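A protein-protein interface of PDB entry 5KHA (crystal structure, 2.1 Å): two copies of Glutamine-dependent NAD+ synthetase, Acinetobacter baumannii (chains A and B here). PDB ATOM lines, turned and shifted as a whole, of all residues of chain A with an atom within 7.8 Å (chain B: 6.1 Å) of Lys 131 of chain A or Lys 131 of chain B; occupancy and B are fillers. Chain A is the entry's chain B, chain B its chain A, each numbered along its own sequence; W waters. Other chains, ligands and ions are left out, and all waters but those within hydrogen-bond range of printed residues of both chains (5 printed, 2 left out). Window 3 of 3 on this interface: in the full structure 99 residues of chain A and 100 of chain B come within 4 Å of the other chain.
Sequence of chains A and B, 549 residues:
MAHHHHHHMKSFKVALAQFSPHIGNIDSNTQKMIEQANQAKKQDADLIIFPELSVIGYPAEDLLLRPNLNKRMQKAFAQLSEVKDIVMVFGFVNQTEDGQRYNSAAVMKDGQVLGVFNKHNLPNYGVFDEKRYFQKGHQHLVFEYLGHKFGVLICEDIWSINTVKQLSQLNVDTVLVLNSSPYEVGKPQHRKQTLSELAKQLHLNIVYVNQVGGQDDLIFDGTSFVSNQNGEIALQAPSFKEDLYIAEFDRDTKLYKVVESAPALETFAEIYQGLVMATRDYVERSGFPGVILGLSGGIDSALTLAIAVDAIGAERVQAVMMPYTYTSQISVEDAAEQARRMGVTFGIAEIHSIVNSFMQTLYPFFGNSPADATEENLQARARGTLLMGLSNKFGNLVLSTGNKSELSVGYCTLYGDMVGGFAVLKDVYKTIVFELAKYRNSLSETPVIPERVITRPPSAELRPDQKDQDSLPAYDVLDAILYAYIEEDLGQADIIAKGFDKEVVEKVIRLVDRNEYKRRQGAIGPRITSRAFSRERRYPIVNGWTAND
Lys 131 of chain A touches just these residues of chain B: Asn 124 and Lys 131.
Of chain A, only Asn 124 and Lys 131 come within 4 Å of Lys 131 of chain B.
Of the printed residues of chain B, Tyr 125 of chain A touches Arg 132.
Of the printed residues of chain B, Asp 129 of chain A touches Asp 129 (3.8 Å).
Printed residues of chain B within 4 Å of Asn 124 of chain A: Asn 124, Lys 131 and Arg 132.
Glu 130 of chain B touches none of the printed residues of chain A.
Phe 128 of chain A touches none of the printed residues of chain B.
The nearest printed residue of chain B that does not touch Lys 131 of chain A is Gln 135 of chain B (6.2 Å).
The nearest printed residue of chain A that does not touch Lys 131 of chain B is Tyr 125 of chain A (6.2 Å).
Water W3 bridges the backbone carbonyl oxygen (O) of Lys 131 of chain A and the side-chain amino group (NZ) of Lys 131 of chain B.
Water W1 lies within hydrogen-bond range of the backbone carbonyl oxygen of Arg 132 of chain A and the backbone carbonyl oxygen of Asn 124 of chain B.
Water W4 lies within hydrogen-bond range of the guanidinium group (NH1) of Arg 132 of chain A, the side-chain carboxylate (OD1) of Asp 129 of chain B and the side-chain amide nitrogen (ND2) of Asn 124 of chain B.
Water W2 lies within hydrogen-bond range of the backbone carbonyl oxygen of Arg 132 of chain B (2.8 Å) and the backbone carbonyl oxygen of Asn 124 of chain A (3.4 Å).
Water W5 lies within hydrogen-bond range of ND2 of Asn 124 of chain B (2.8 Å), OD1 of Asp 129 of chain B (2.8 Å), ND2 of Asn 124 of chain A (2.9 Å) and OD1 of Asp 129 of chain A (2.9 Å).
The backbone NH (N) of Arg 132 of chain B lies close to the side-chain amide nitrogen (ND2) of Asn 124 of chain A (3.4 Å).
The side-chain amide nitrogen (ND2) of Asn 124 of chain B lies close to the backbone NH (N) of Arg 132 of chain A (3.2 Å).
Asn 124 of chain B touches Asn 124 of chain A (ND2 to OD1, 3.8 Å).
Lys 131 of chain B touches Asn 124 of chain A (C to ND2, 3.6 Å).
Tyr 125 of chain A touches Arg 132 of chain B (C to NH1, 3.9 Å).
Asp 129 of chain A touches Asp 129 of chain B.
Lys 131 of chain A touches Asn 124 of chain B (C to ND2, 3.6 Å).
CB of Lys 131 of chain A touches CD of Lys 131 of chain B (3.98 Å).
OD1 of Asn 124 of chain B lies within hydrogen-bond range of N of Lys 131 of chain B, 2.9 Å away.
NE of Arg 132 of chain A lies close to OH of Tyr 133 of chain A (3.5 Å).
OD1 of Asn 124 of chain A lies within hydrogen-bond range of N of Lys 131 of chain A (2.8 Å).
The guanidinium group of Arg 132 of chain B sits close to the side-chain hydroxyl of Tyr 133 of chain B, 3.4 Å away.
The backbone NH (N) of Glu 130 of chain A sits at hydrogen-bond distance from the side-chain amide oxygen (OD1) of Asn 124 of chain A (3.2 Å).
The backbone NH (N) of Glu 130 of chain B lies within hydrogen-bond range of the side-chain amide oxygen (OD1) of Asn 124 of chain B (3.3 Å).
Asn 124 of chain B touches its own counterpart, Asn 124 of chain A.
Asn 124 of chain A touches Arg 132 of chain B, and with the chains exchanged Arg 132 of chain A touches Asn 124 of chain B.
Asp 129 of chain A touches its own counterpart, Asp 129 of chain B.
Lys 131 of chain B touches its own counterpart, Lys 131 of chain A.
10 positions are printed for both chains.
Of the 8 pairs that touch across the chains among the printed residues, 7 have their exchanged pair printed and touching as well.
Along chain B the printed residues that touch a printed residue of chain A span positions 124 to 132.
Among the printed residues, no Asp or Glu carboxylate lies within 4 Å of a Lys or Arg side-chain nitrogen of the other chain.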
ATOM      1  N   LEU A  65     -32.474   8.893   8.173  1.00  0.00           N
ATOM      2  CA  LEU A  65     -32.425  10.127   7.407  1.00  0.00           C
ATOM      3  C   LEU A  65     -32.797  11.359   8.220  1.00  0.00           C
ATOM      4  O   LEU A  65     -32.827  12.457   7.663  1.00  0.00           O
ATOM      5  CB  LEU A  65     -33.356  10.027   6.197  1.00  0.00           C
ATOM      6  CG  LEU A  65     -33.044   8.910   5.209  1.00  0.00           C
ATOM      7  CD1 LEU A  65     -34.180   8.794   4.205  1.00  0.00           C
ATOM      8  CD2 LEU A  65     -31.740   9.211   4.501  1.00  0.00           C
ATOM      9  N   ARG A 101     -23.006   9.778   5.110  1.00  0.00           N
ATOM     10  CA  ARG A 101     -23.366   8.888   6.213  1.00  0.00           C
ATOM     11  C   ARG A 101     -22.870   7.481   5.908  1.00  0.00           C
ATOM     12  O   ARG A 101     -23.044   6.979   4.786  1.00  0.00           O
ATOM     13  CB  ARG A 101     -24.880   8.850   6.477  1.00  0.00           C
ATOM     14  CG  ARG A 101     -25.384   9.909   7.448  1.00  0.00           C
ATOM     15  CD  ARG A 101     -26.883   9.761   7.629  1.00  0.00           C
ATOM     16  NE  ARG A 101     -27.490   9.305   6.384  1.00  0.00           N
ATOM     17  CZ  ARG A 101     -28.107  10.100   5.517  1.00  0.00           C
ATOM     18  NH1 ARG A 101     -28.244  11.397   5.772  1.00  0.00           N
ATOM     19  NH2 ARG A 101     -28.604   9.590   4.399  1.00  0.00           N
ATOM     20  N   HIS A 120     -18.018  -1.624   3.814  1.00  0.00           N
ATOM     21  CA  HIS A 120     -17.666  -1.547   2.395  1.00  0.00           C
ATOM     22  C   HIS A 120     -18.791  -2.007   1.478  1.00  0.00           C
ATOM     23  O   HIS A 120     -18.993  -1.435   0.401  1.00  0.00           O
ATOM     24  CB  HIS A 120     -16.423  -2.401   2.080  1.00  0.00           C
ATOM     25  CG  HIS A 120     -15.148  -1.892   2.689  1.00  0.00           C
ATOM     26  ND1 HIS A 120     -13.905  -2.201   2.176  1.00  0.00           N
ATOM     27  CD2 HIS A 120     -14.923  -1.131   3.786  1.00  0.00           C
ATOM     28  CE1 HIS A 120     -12.968  -1.648   2.932  1.00  0.00           C
ATOM     29  NE2 HIS A 120     -13.559  -1.000   3.920  1.00  0.00           N
ATOM     30  N   ASN A 121     -19.500  -3.057   1.862  1.00  0.00           N
ATOM     31  CA  ASN A 121     -20.459  -3.734   0.994  1.00  0.00           C
ATOM     32  C   ASN A 121     -21.862  -3.473   1.532  1.00  0.00           C
ATOM     33  O   ASN A 121     -22.259  -4.067   2.530  1.00  0.00           O
ATOM     34  CB  ASN A 121     -20.156  -5.226   0.938  1.00  0.00           C
ATOM     35  CG  ASN A 121     -18.844  -5.521   0.269  1.00  0.00           C
ATOM     36  OD1 ASN A 121     -18.793  -5.659  -0.946  1.00  0.00           O
ATOM     37  ND2 ASN A 121     -17.770  -5.605   1.048  1.00  0.00           N
ATOM     38  N   LEU A 122     -22.601  -2.577   0.869  1.00  0.00           N
ATOM     39  CA  LEU A 122     -23.948  -2.174   1.268  1.00  0.00           C
ATOM     40  C   LEU A 122     -25.024  -2.993   0.560  1.00  0.00           C
ATOM     41  O   LEU A 122     -25.329  -2.739  -0.615  1.00  0.00           O
ATOM     42  CB  LEU A 122     -24.167  -0.696   0.971  1.00  0.00           C
ATOM     43  CG  LEU A 122     -23.160   0.261   1.587  1.00  0.00           C
ATOM     44  CD1 LEU A 122     -23.414   1.680   1.068  1.00  0.00           C
ATOM     45  CD2 LEU A 122     -23.232   0.194   3.103  1.00  0.00           C
ATOM     46  N   PRO A 123     -25.659  -3.943   1.242  1.00  0.00           N
ATOM     47  CA  PRO A 123     -26.692  -4.747   0.578  1.00  0.00           C
ATOM     48  C   PRO A 123     -27.884  -3.895   0.147  1.00  0.00           C
ATOM     49  O   PRO A 123     -28.445  -3.121   0.927  1.00  0.00           O
ATOM     50  CB  PRO A 123     -27.085  -5.774   1.649  1.00  0.00           C
ATOM     51  CG  PRO A 123     -26.774  -5.104   2.946  1.00  0.00           C
ATOM     52  CD  PRO A 123     -25.560  -4.234   2.685  1.00  0.00           C
ATOM     53  N   ASN A 124     -28.278  -4.054  -1.105  1.00  0.00           N
ATOM     54  CA  ASN A 124     -29.468  -3.385  -1.608  1.00  0.00           C
ATOM     55  C   ASN A 124     -30.259  -4.377  -2.454  1.00  0.00           C
ATOM     56  O   ASN A 124     -30.594  -4.127  -3.611  1.00  0.00           O
ATOM     57  CB  ASN A 124     -29.097  -2.124  -2.401  1.00  0.00           C
ATOM     58  CG  ASN A 124     -30.107  -0.995  -2.207  1.00  0.00           C
ATOM     59  OD1 ASN A 124     -30.016  -0.221  -1.245  1.00  0.00           O
ATOM     60  ND2 ASN A 124     -31.086  -0.912  -3.102  1.00  0.00           N
ATOM     61  N   TYR A 125     -30.547  -5.536  -1.866  1.00  0.00           N
ATOM     62  CA  TYR A 125     -31.288  -6.596  -2.520  1.00  0.00           C
ATOM     63  C   TYR A 125     -32.196  -7.216  -1.471  1.00  0.00           C
ATOM     64  O   TYR A 125     -31.925  -7.129  -0.278  1.00  0.00           O
ATOM     65  CB  TYR A 125     -30.342  -7.668  -3.134  1.00  0.00           C
ATOM     66  CG  TYR A 125     -29.477  -8.328  -2.087  1.00  0.00           C
ATOM     67  CD1 TYR A 125     -28.196  -7.857  -1.813  1.00  0.00           C
ATOM     68  CD2 TYR A 125     -29.963  -9.388  -1.329  1.00  0.00           C
ATOM     69  CE1 TYR A 125     -27.413  -8.445  -0.812  1.00  0.00           C
ATOM     70  CE2 TYR A 125     -29.199  -9.976  -0.334  1.00  0.00           C
ATOM     71  CZ  TYR A 125     -27.933  -9.504  -0.074  1.00  0.00           C
ATOM     72  OH  TYR A 125     -27.189 -10.111   0.917  1.00  0.00           O
ATOM     73  N   PHE A 128     -32.908  -5.791   2.046  1.00  0.00           N
ATOM     74  CA  PHE A 128     -31.940  -4.756   2.382  1.00  0.00           C
ATOM     75  C   PHE A 128     -32.086  -3.552   1.461  1.00  0.00           C
ATOM     76  O   PHE A 128     -32.314  -3.706   0.258  1.00  0.00           O
ATOM     77  CB  PHE A 128     -30.510  -5.314   2.300  1.00  0.00           C
ATOM     78  CG  PHE A 128     -30.300  -6.560   3.140  1.00  0.00           C
ATOM     79  CD1 PHE A 128     -30.234  -6.470   4.530  1.00  0.00           C
ATOM     80  CD2 PHE A 128     -30.172  -7.813   2.542  1.00  0.00           C
ATOM     81  CE1 PHE A 128     -30.042  -7.605   5.316  1.00  0.00           C
ATOM     82  CE2 PHE A 128     -29.987  -8.952   3.311  1.00  0.00           C
ATOM     83  CZ  PHE A 128     -29.917  -8.850   4.703  1.00  0.00           C
ATOM     84  N   ASP A 129     -31.952  -2.352   2.029  1.00  0.00           N
ATOM     85  CA  ASP A 129     -32.021  -1.110   1.253  1.00  0.00           C
ATOM     86  C   ASP A 129     -30.950  -0.121   1.693  1.00  0.00           C
ATOM     87  O   ASP A 129     -31.200   1.084   1.785  1.00  0.00           O
ATOM     88  CB  ASP A 129     -33.397  -0.453   1.375  1.00  0.00           C
ATOM     89  CG  ASP A 129     -34.482  -1.282   0.752  1.00  0.00           C
ATOM     90  OD1 ASP A 129     -34.645  -1.223  -0.493  1.00  0.00           O
ATOM     91  OD2 ASP A 129     -35.165  -2.006   1.516  1.00  0.00           O
ATOM     92  N   GLU A 130     -29.728  -0.601   1.923  1.00  0.00           N
ATOM     93  CA  GLU A 130     -28.743   0.231   2.598  1.00  0.00           C
ATOM     94  C   GLU A 130     -28.213   1.366   1.735  1.00  0.00           C
ATOM     95  O   GLU A 130     -27.695   2.340   2.286  1.00  0.00           O
ATOM     96  CB  GLU A 130     -27.601  -0.638   3.108  1.00  0.00           C
ATOM     97  CG  GLU A 130     -28.085  -1.499   4.269  1.00  0.00           C
ATOM     98  CD  GLU A 130     -26.963  -1.984   5.132  1.00  0.00           C
ATOM     99  OE1 GLU A 130     -25.805  -1.552   4.912  1.00  0.00           O
ATOM    100  OE2 GLU A 130     -27.235  -2.818   6.011  1.00  0.00           O
ATOM    101  N   LYS A 131     -28.343   1.291   0.411  1.00  0.00           N
ATOM    102  CA  LYS A 131     -27.935   2.423  -0.419  1.00  0.00           C
ATOM    103  C   LYS A 131     -28.961   3.547  -0.417  1.00  0.00           C
ATOM    104  O   LYS A 131     -28.696   4.613  -0.980  1.00  0.00           O
ATOM    105  CB  LYS A 131     -27.650   1.942  -1.843  1.00  0.00           C
ATOM    106  CG  LYS A 131     -26.457   0.972  -1.851  1.00  0.00           C
ATOM    107  CD  LYS A 131     -26.111   0.471  -3.222  1.00  0.00           C
ATOM    108  CE  LYS A 131     -24.816  -0.357  -3.180  1.00  0.00           C
ATOM    109  NZ  LYS A 131     -24.646  -1.132  -4.438  1.00  0.00           N
ATOM    110  N   ARG A 132     -30.124   3.343   0.216  1.00  0.00           N
ATOM    111  CA  ARG A 132     -31.016   4.462   0.513  1.00  0.00           C
ATOM    112  C   ARG A 132     -30.434   5.376   1.583  1.00  0.00           C
ATOM    113  O   ARG A 132     -30.822   6.550   1.658  1.00  0.00           O
ATOM    114  CB  ARG A 132     -32.384   3.922   0.962  1.00  0.00           C
ATOM    115  CG  ARG A 132     -33.490   4.966   1.223  1.00  0.00           C
ATOM    116  CD  ARG A 132     -34.792   4.219   1.574  1.00  0.00           C
ATOM    117  NE  ARG A 132     -35.923   5.099   1.865  1.00  0.00           N
ATOM    118  CZ  ARG A 132     -36.786   5.567   0.967  1.00  0.00           C
ATOM    119  NH1 ARG A 132     -36.677   5.276  -0.328  1.00  0.00           N
ATOM    120  NH2 ARG A 132     -37.775   6.350   1.369  1.00  0.00           N
ATOM    121  N   TYR A 133     -29.515   4.854   2.408  1.00  0.00           N
ATOM    122  CA  TYR A 133     -29.051   5.502   3.635  1.00  0.00           C
ATOM    123  C   TYR A 133     -27.559   5.778   3.698  1.00  0.00           C
ATOM    124  O   TYR A 133     -27.170   6.766   4.324  1.00  0.00           O
ATOM    125  CB  TYR A 133     -29.419   4.642   4.866  1.00  0.00           C
ATOM    126  CG  TYR A 133     -30.882   4.306   4.873  1.00  0.00           C
ATOM    127  CD1 TYR A 133     -31.829   5.319   4.909  1.00  0.00           C
ATOM    128  CD2 TYR A 133     -31.327   2.988   4.813  1.00  0.00           C
ATOM    129  CE1 TYR A 133     -33.164   5.044   4.892  1.00  0.00           C
ATOM    130  CE2 TYR A 133     -32.692   2.699   4.792  1.00  0.00           C
ATOM    131  CZ  TYR A 133     -33.601   3.740   4.838  1.00  0.00           C
ATOM    132  OH  TYR A 133     -34.965   3.513   4.820  1.00  0.00           O
ATOM    133  N   PHE A 134     -26.706   4.934   3.101  1.00  0.00           N
ATOM    134  CA  PHE A 134     -25.279   5.008   3.400  1.00  0.00           C
ATOM    135  C   PHE A 134     -24.461   5.095   2.133  1.00  0.00           C
ATOM    136  O   PHE A 134     -24.881   4.644   1.068  1.00  0.00           O
ATOM    137  CB  PHE A 134     -24.764   3.791   4.218  1.00  0.00           C
ATOM    138  CG  PHE A 134     -25.555   3.509   5.469  1.00  0.00           C
ATOM    139  CD1 PHE A 134     -26.293   2.335   5.589  1.00  0.00           C
ATOM    140  CD2 PHE A 134     -25.542   4.404   6.526  1.00  0.00           C
ATOM    141  CE1 PHE A 134     -27.019   2.057   6.745  1.00  0.00           C
ATOM    142  CE2 PHE A 134     -26.255   4.146   7.686  1.00  0.00           C
ATOM    143  CZ  PHE A 134     -26.998   2.972   7.804  1.00  0.00           C
ATOM    144  N   GLN A 135     -23.279   5.689   2.276  1.00  0.00           N
ATOM    145  CA  GLN A 135     -22.218   5.604   1.289  1.00  0.00           C
ATOM    146  C   GLN A 135     -21.242   4.535   1.772  1.00  0.00           C
ATOM    147  O   GLN A 135     -21.149   4.251   2.968  1.00  0.00           O
ATOM    148  CB  GLN A 135     -21.509   6.958   1.117  1.00  0.00           C
ATOM    149  CG  GLN A 135     -22.254   7.935   0.193  1.00  0.00           C
ATOM    150  CD  GLN A 135     -23.572   8.429   0.789  1.00  0.00           C
ATOM    151  OE1 GLN A 135     -23.590   9.166   1.779  1.00  0.00           O
ATOM    152  NE2 GLN A 135     -24.679   8.012   0.188  1.00  0.00           N
ATOM    153  N   LYS A 136     -20.523   3.929   0.838  1.00  0.00           N
ATOM    154  CA  LYS A 136     -19.667   2.803   1.178  1.00  0.00           C
ATOM    155  C   LYS A 136     -18.279   3.247   1.639  1.00  0.00           C
ATOM    156  O   LYS A 136     -17.737   4.267   1.188  1.00  0.00           O
ATOM    157  CB  LYS A 136     -19.560   1.849  -0.014  1.00  0.00           C
ATOM    158  CG  LYS A 136     -18.776   2.376  -1.193  1.00  0.00           C
ATOM    159  CD  LYS A 136     -19.013   1.480  -2.410  1.00  0.00           C
ATOM    160  CE  LYS A 136     -17.995   0.359  -2.493  1.00  0.00           C
ATOM    161  NZ  LYS A 136     -16.635   0.929  -2.704  1.00  0.00           N
ATOM    162  N   LEU B 122     -28.338   7.125 -10.397  1.00  0.00           N
ATOM    163  CA  LEU B 122     -29.429   6.203 -10.084  1.00  0.00           C
ATOM    164  C   LEU B 122     -30.139   6.648  -8.809  1.00  0.00           C
ATOM    165  O   LEU B 122     -29.589   6.463  -7.714  1.00  0.00           O
ATOM    166  CB  LEU B 122     -28.896   4.786  -9.913  1.00  0.00           C
ATOM    167  CG  LEU B 122     -28.104   4.191 -11.083  1.00  0.00           C
ATOM    168  CD1 LEU B 122     -27.471   2.844 -10.693  1.00  0.00           C
ATOM    169  CD2 LEU B 122     -29.011   4.053 -12.299  1.00  0.00           C
ATOM    170  N   PRO B 123     -31.344   7.208  -8.887  1.00  0.00           N
ATOM    171  CA  PRO B 123     -32.029   7.650  -7.659  1.00  0.00           C
ATOM    172  C   PRO B 123     -32.363   6.473  -6.750  1.00  0.00           C
ATOM    173  O   PRO B 123     -32.936   5.471  -7.183  1.00  0.00           O
ATOM    174  CB  PRO B 123     -33.295   8.339  -8.184  1.00  0.00           C
ATOM    175  CG  PRO B 123     -33.549   7.680  -9.507  1.00  0.00           C
ATOM    176  CD  PRO B 123     -32.198   7.336 -10.079  1.00  0.00           C
ATOM    177  N   ASN B 124     -31.998   6.605  -5.481  1.00  0.00           N
ATOM    178  CA  ASN B 124     -32.339   5.622  -4.462  1.00  0.00           C
ATOM    179  C   ASN B 124     -32.816   6.361  -3.211  1.00  0.00           C
ATOM    180  O   ASN B 124     -32.260   6.235  -2.122  1.00  0.00           O
ATOM    181  CB  ASN B 124     -31.167   4.686  -4.172  1.00  0.00           C
ATOM    182  CG  ASN B 124     -31.637   3.270  -3.849  1.00  0.00           C
ATOM    183  OD1 ASN B 124     -31.912   2.487  -4.747  1.00  0.00           O
ATOM    184  ND2 ASN B 124     -31.735   2.946  -2.566  1.00  0.00           N
ATOM    185  N   ASP B 129     -35.889   3.269  -6.173  1.00  0.00           N
ATOM    186  CA  ASP B 129     -35.024   2.205  -5.667  1.00  0.00           C
ATOM    187  C   ASP B 129     -34.110   1.662  -6.766  1.00  0.00           C
ATOM    188  O   ASP B 129     -33.932   0.449  -6.900  1.00  0.00           O
ATOM    189  CB  ASP B 129     -35.844   1.063  -5.080  1.00  0.00           C
ATOM    190  CG  ASP B 129     -36.582   1.465  -3.847  1.00  0.00           C
ATOM    191  OD1 ASP B 129     -35.956   1.510  -2.760  1.00  0.00           O
ATOM    192  OD2 ASP B 129     -37.798   1.698  -3.959  1.00  0.00           O
ATOM    193  N   GLU B 130     -33.516   2.542  -7.576  1.00  0.00           N
ATOM    194  CA  GLU B 130     -32.854   2.056  -8.777  1.00  0.00           C
ATOM    195  C   GLU B 130     -31.557   1.314  -8.486  1.00  0.00           C
ATOM    196  O   GLU B 130     -31.103   0.549  -9.339  1.00  0.00           O
ATOM    197  CB  GLU B 130     -32.623   3.210  -9.755  1.00  0.00           C
ATOM    198  CG  GLU B 130     -33.966   3.675 -10.331  1.00  0.00           C
ATOM    199  CD  GLU B 130     -33.849   4.425 -11.640  1.00  0.00           C
ATOM    200  OE1 GLU B 130     -32.723   4.488 -12.185  1.00  0.00           O
ATOM    201  OE2 GLU B 130     -34.890   4.959 -12.115  1.00  0.00           O
ATOM    202  N   LYS B 131     -30.956   1.493  -7.314  1.00  0.00           N
ATOM    203  CA  LYS B 131     -29.770   0.702  -6.996  1.00  0.00           C
ATOM    204  C   LYS B 131     -30.113  -0.723  -6.575  1.00  0.00           C
ATOM    205  O   LYS B 131     -29.199  -1.537  -6.365  1.00  0.00           O
ATOM    206  CB  LYS B 131     -28.944   1.418  -5.929  1.00  0.00           C
ATOM    207  CG  LYS B 131     -28.406   2.733  -6.472  1.00  0.00           C
ATOM    208  CD  LYS B 131     -27.567   3.501  -5.499  1.00  0.00           C
ATOM    209  CE  LYS B 131     -26.943   4.705  -6.224  1.00  0.00           C
ATOM    210  NZ  LYS B 131     -26.424   5.713  -5.285  1.00  0.00           N
ATOM    211  N   ARG B 132     -31.408  -1.037  -6.451  1.00  0.00           N
ATOM    212  CA  ARG B 132     -31.858  -2.422  -6.350  1.00  0.00           C
ATOM    213  C   ARG B 132     -31.713  -3.156  -7.673  1.00  0.00           C
ATOM    214  O   ARG B 132     -31.591  -4.385  -7.672  1.00  0.00           O
ATOM    215  CB  ARG B 132     -33.332  -2.469  -5.894  1.00  0.00           C
ATOM    216  CG  ARG B 132     -33.895  -3.886  -5.642  1.00  0.00           C
ATOM    217  CD  ARG B 132     -35.336  -3.773  -5.171  1.00  0.00           C
ATOM    218  NE  ARG B 132     -35.995  -5.067  -4.939  1.00  0.00           N
ATOM    219  CZ  ARG B 132     -35.967  -5.736  -3.791  1.00  0.00           C
ATOM    220  NH1 ARG B 132     -35.286  -5.258  -2.765  1.00  0.00           N
ATOM    221  NH2 ARG B 132     -36.622  -6.888  -3.672  1.00  0.00           N
ATOM    222  N   TYR B 133     -31.704  -2.426  -8.801  1.00  0.00           N
ATOM    223  CA  TYR B 133     -31.813  -3.004 -10.139  1.00  0.00           C
ATOM    224  C   TYR B 133     -30.626  -2.715 -11.053  1.00  0.00           C
ATOM    225  O   TYR B 133     -30.305  -3.547 -11.898  1.00  0.00           O
ATOM    226  CB  TYR B 133     -33.107  -2.509 -10.823  1.00  0.00           C
ATOM    227  CG  TYR B 133     -34.330  -2.759  -9.963  1.00  0.00           C
ATOM    228  CD1 TYR B 133     -34.674  -4.053  -9.598  1.00  0.00           C
ATOM    229  CD2 TYR B 133     -35.136  -1.708  -9.509  1.00  0.00           C
ATOM    230  CE1 TYR B 133     -35.777  -4.300  -8.796  1.00  0.00           C
ATOM    231  CE2 TYR B 133     -36.236  -1.941  -8.696  1.00  0.00           C
ATOM    232  CZ  TYR B 133     -36.551  -3.252  -8.348  1.00  0.00           C
ATOM    233  OH  TYR B 133     -37.633  -3.528  -7.549  1.00  0.00           O
ATOM    234  N   PHE B 134     -29.960  -1.573 -10.913  1.00  0.00           N
ATOM    235  CA  PHE B 134     -29.020  -1.131 -11.935  1.00  0.00           C
ATOM    236  C   PHE B 134     -27.664  -0.770 -11.355  1.00  0.00           C
ATOM    237  O   PHE B 134     -27.528  -0.396 -10.187  1.00  0.00           O
ATOM    238  CB  PHE B 134     -29.538   0.094 -12.708  1.00  0.00           C
ATOM    239  CG  PHE B 134     -30.906  -0.082 -13.325  1.00  0.00           C
ATOM    240  CD1 PHE B 134     -31.989   0.651 -12.859  1.00  0.00           C
ATOM    241  CD2 PHE B 134     -31.096  -0.954 -14.396  1.00  0.00           C
ATOM    242  CE1 PHE B 134     -33.238   0.528 -13.444  1.00  0.00           C
ATOM    243  CE2 PHE B 134     -32.338  -1.085 -14.987  1.00  0.00           C
ATOM    244  CZ  PHE B 134     -33.413  -0.345 -14.515  1.00  0.00           C
ATOM    245  N   GLN B 135     -26.664  -0.877 -12.217  1.00  0.00           N
ATOM    246  CA  GLN B 135     -25.361  -0.278 -12.004  1.00  0.00           C
ATOM    247  C   GLN B 135     -25.301   1.025 -12.791  1.00  0.00           C
ATOM    248  O   GLN B 135     -26.049   1.224 -13.748  1.00  0.00           O
ATOM    249  CB  GLN B 135     -24.229  -1.216 -12.443  1.00  0.00           C
ATOM    250  CG  GLN B 135     -23.863  -2.261 -11.394  1.00  0.00           C
ATOM    251  CD  GLN B 135     -24.959  -3.296 -11.190  1.00  0.00           C
ATOM    252  OE1 GLN B 135     -25.560  -3.372 -10.117  1.00  0.00           O
ATOM    253  NE2 GLN B 135     -25.223  -4.097 -12.222  1.00  0.00           N
HETATM  254  O   HOH W   1     -32.577   8.258   0.640  1.00  0.00           O
HETATM  255  O   HOH W   2     -31.432  -6.515  -5.916  1.00  0.00           O
HETATM  256  O   HOH W   3     -27.750   5.989  -2.747  1.00  0.00           O
HETATM  257  O   HOH W   4     -34.904   4.039  -1.950  1.00  0.00           O
HETATM  258  O   HOH W   5     -33.304   0.668  -2.241  1.00  0.00           O
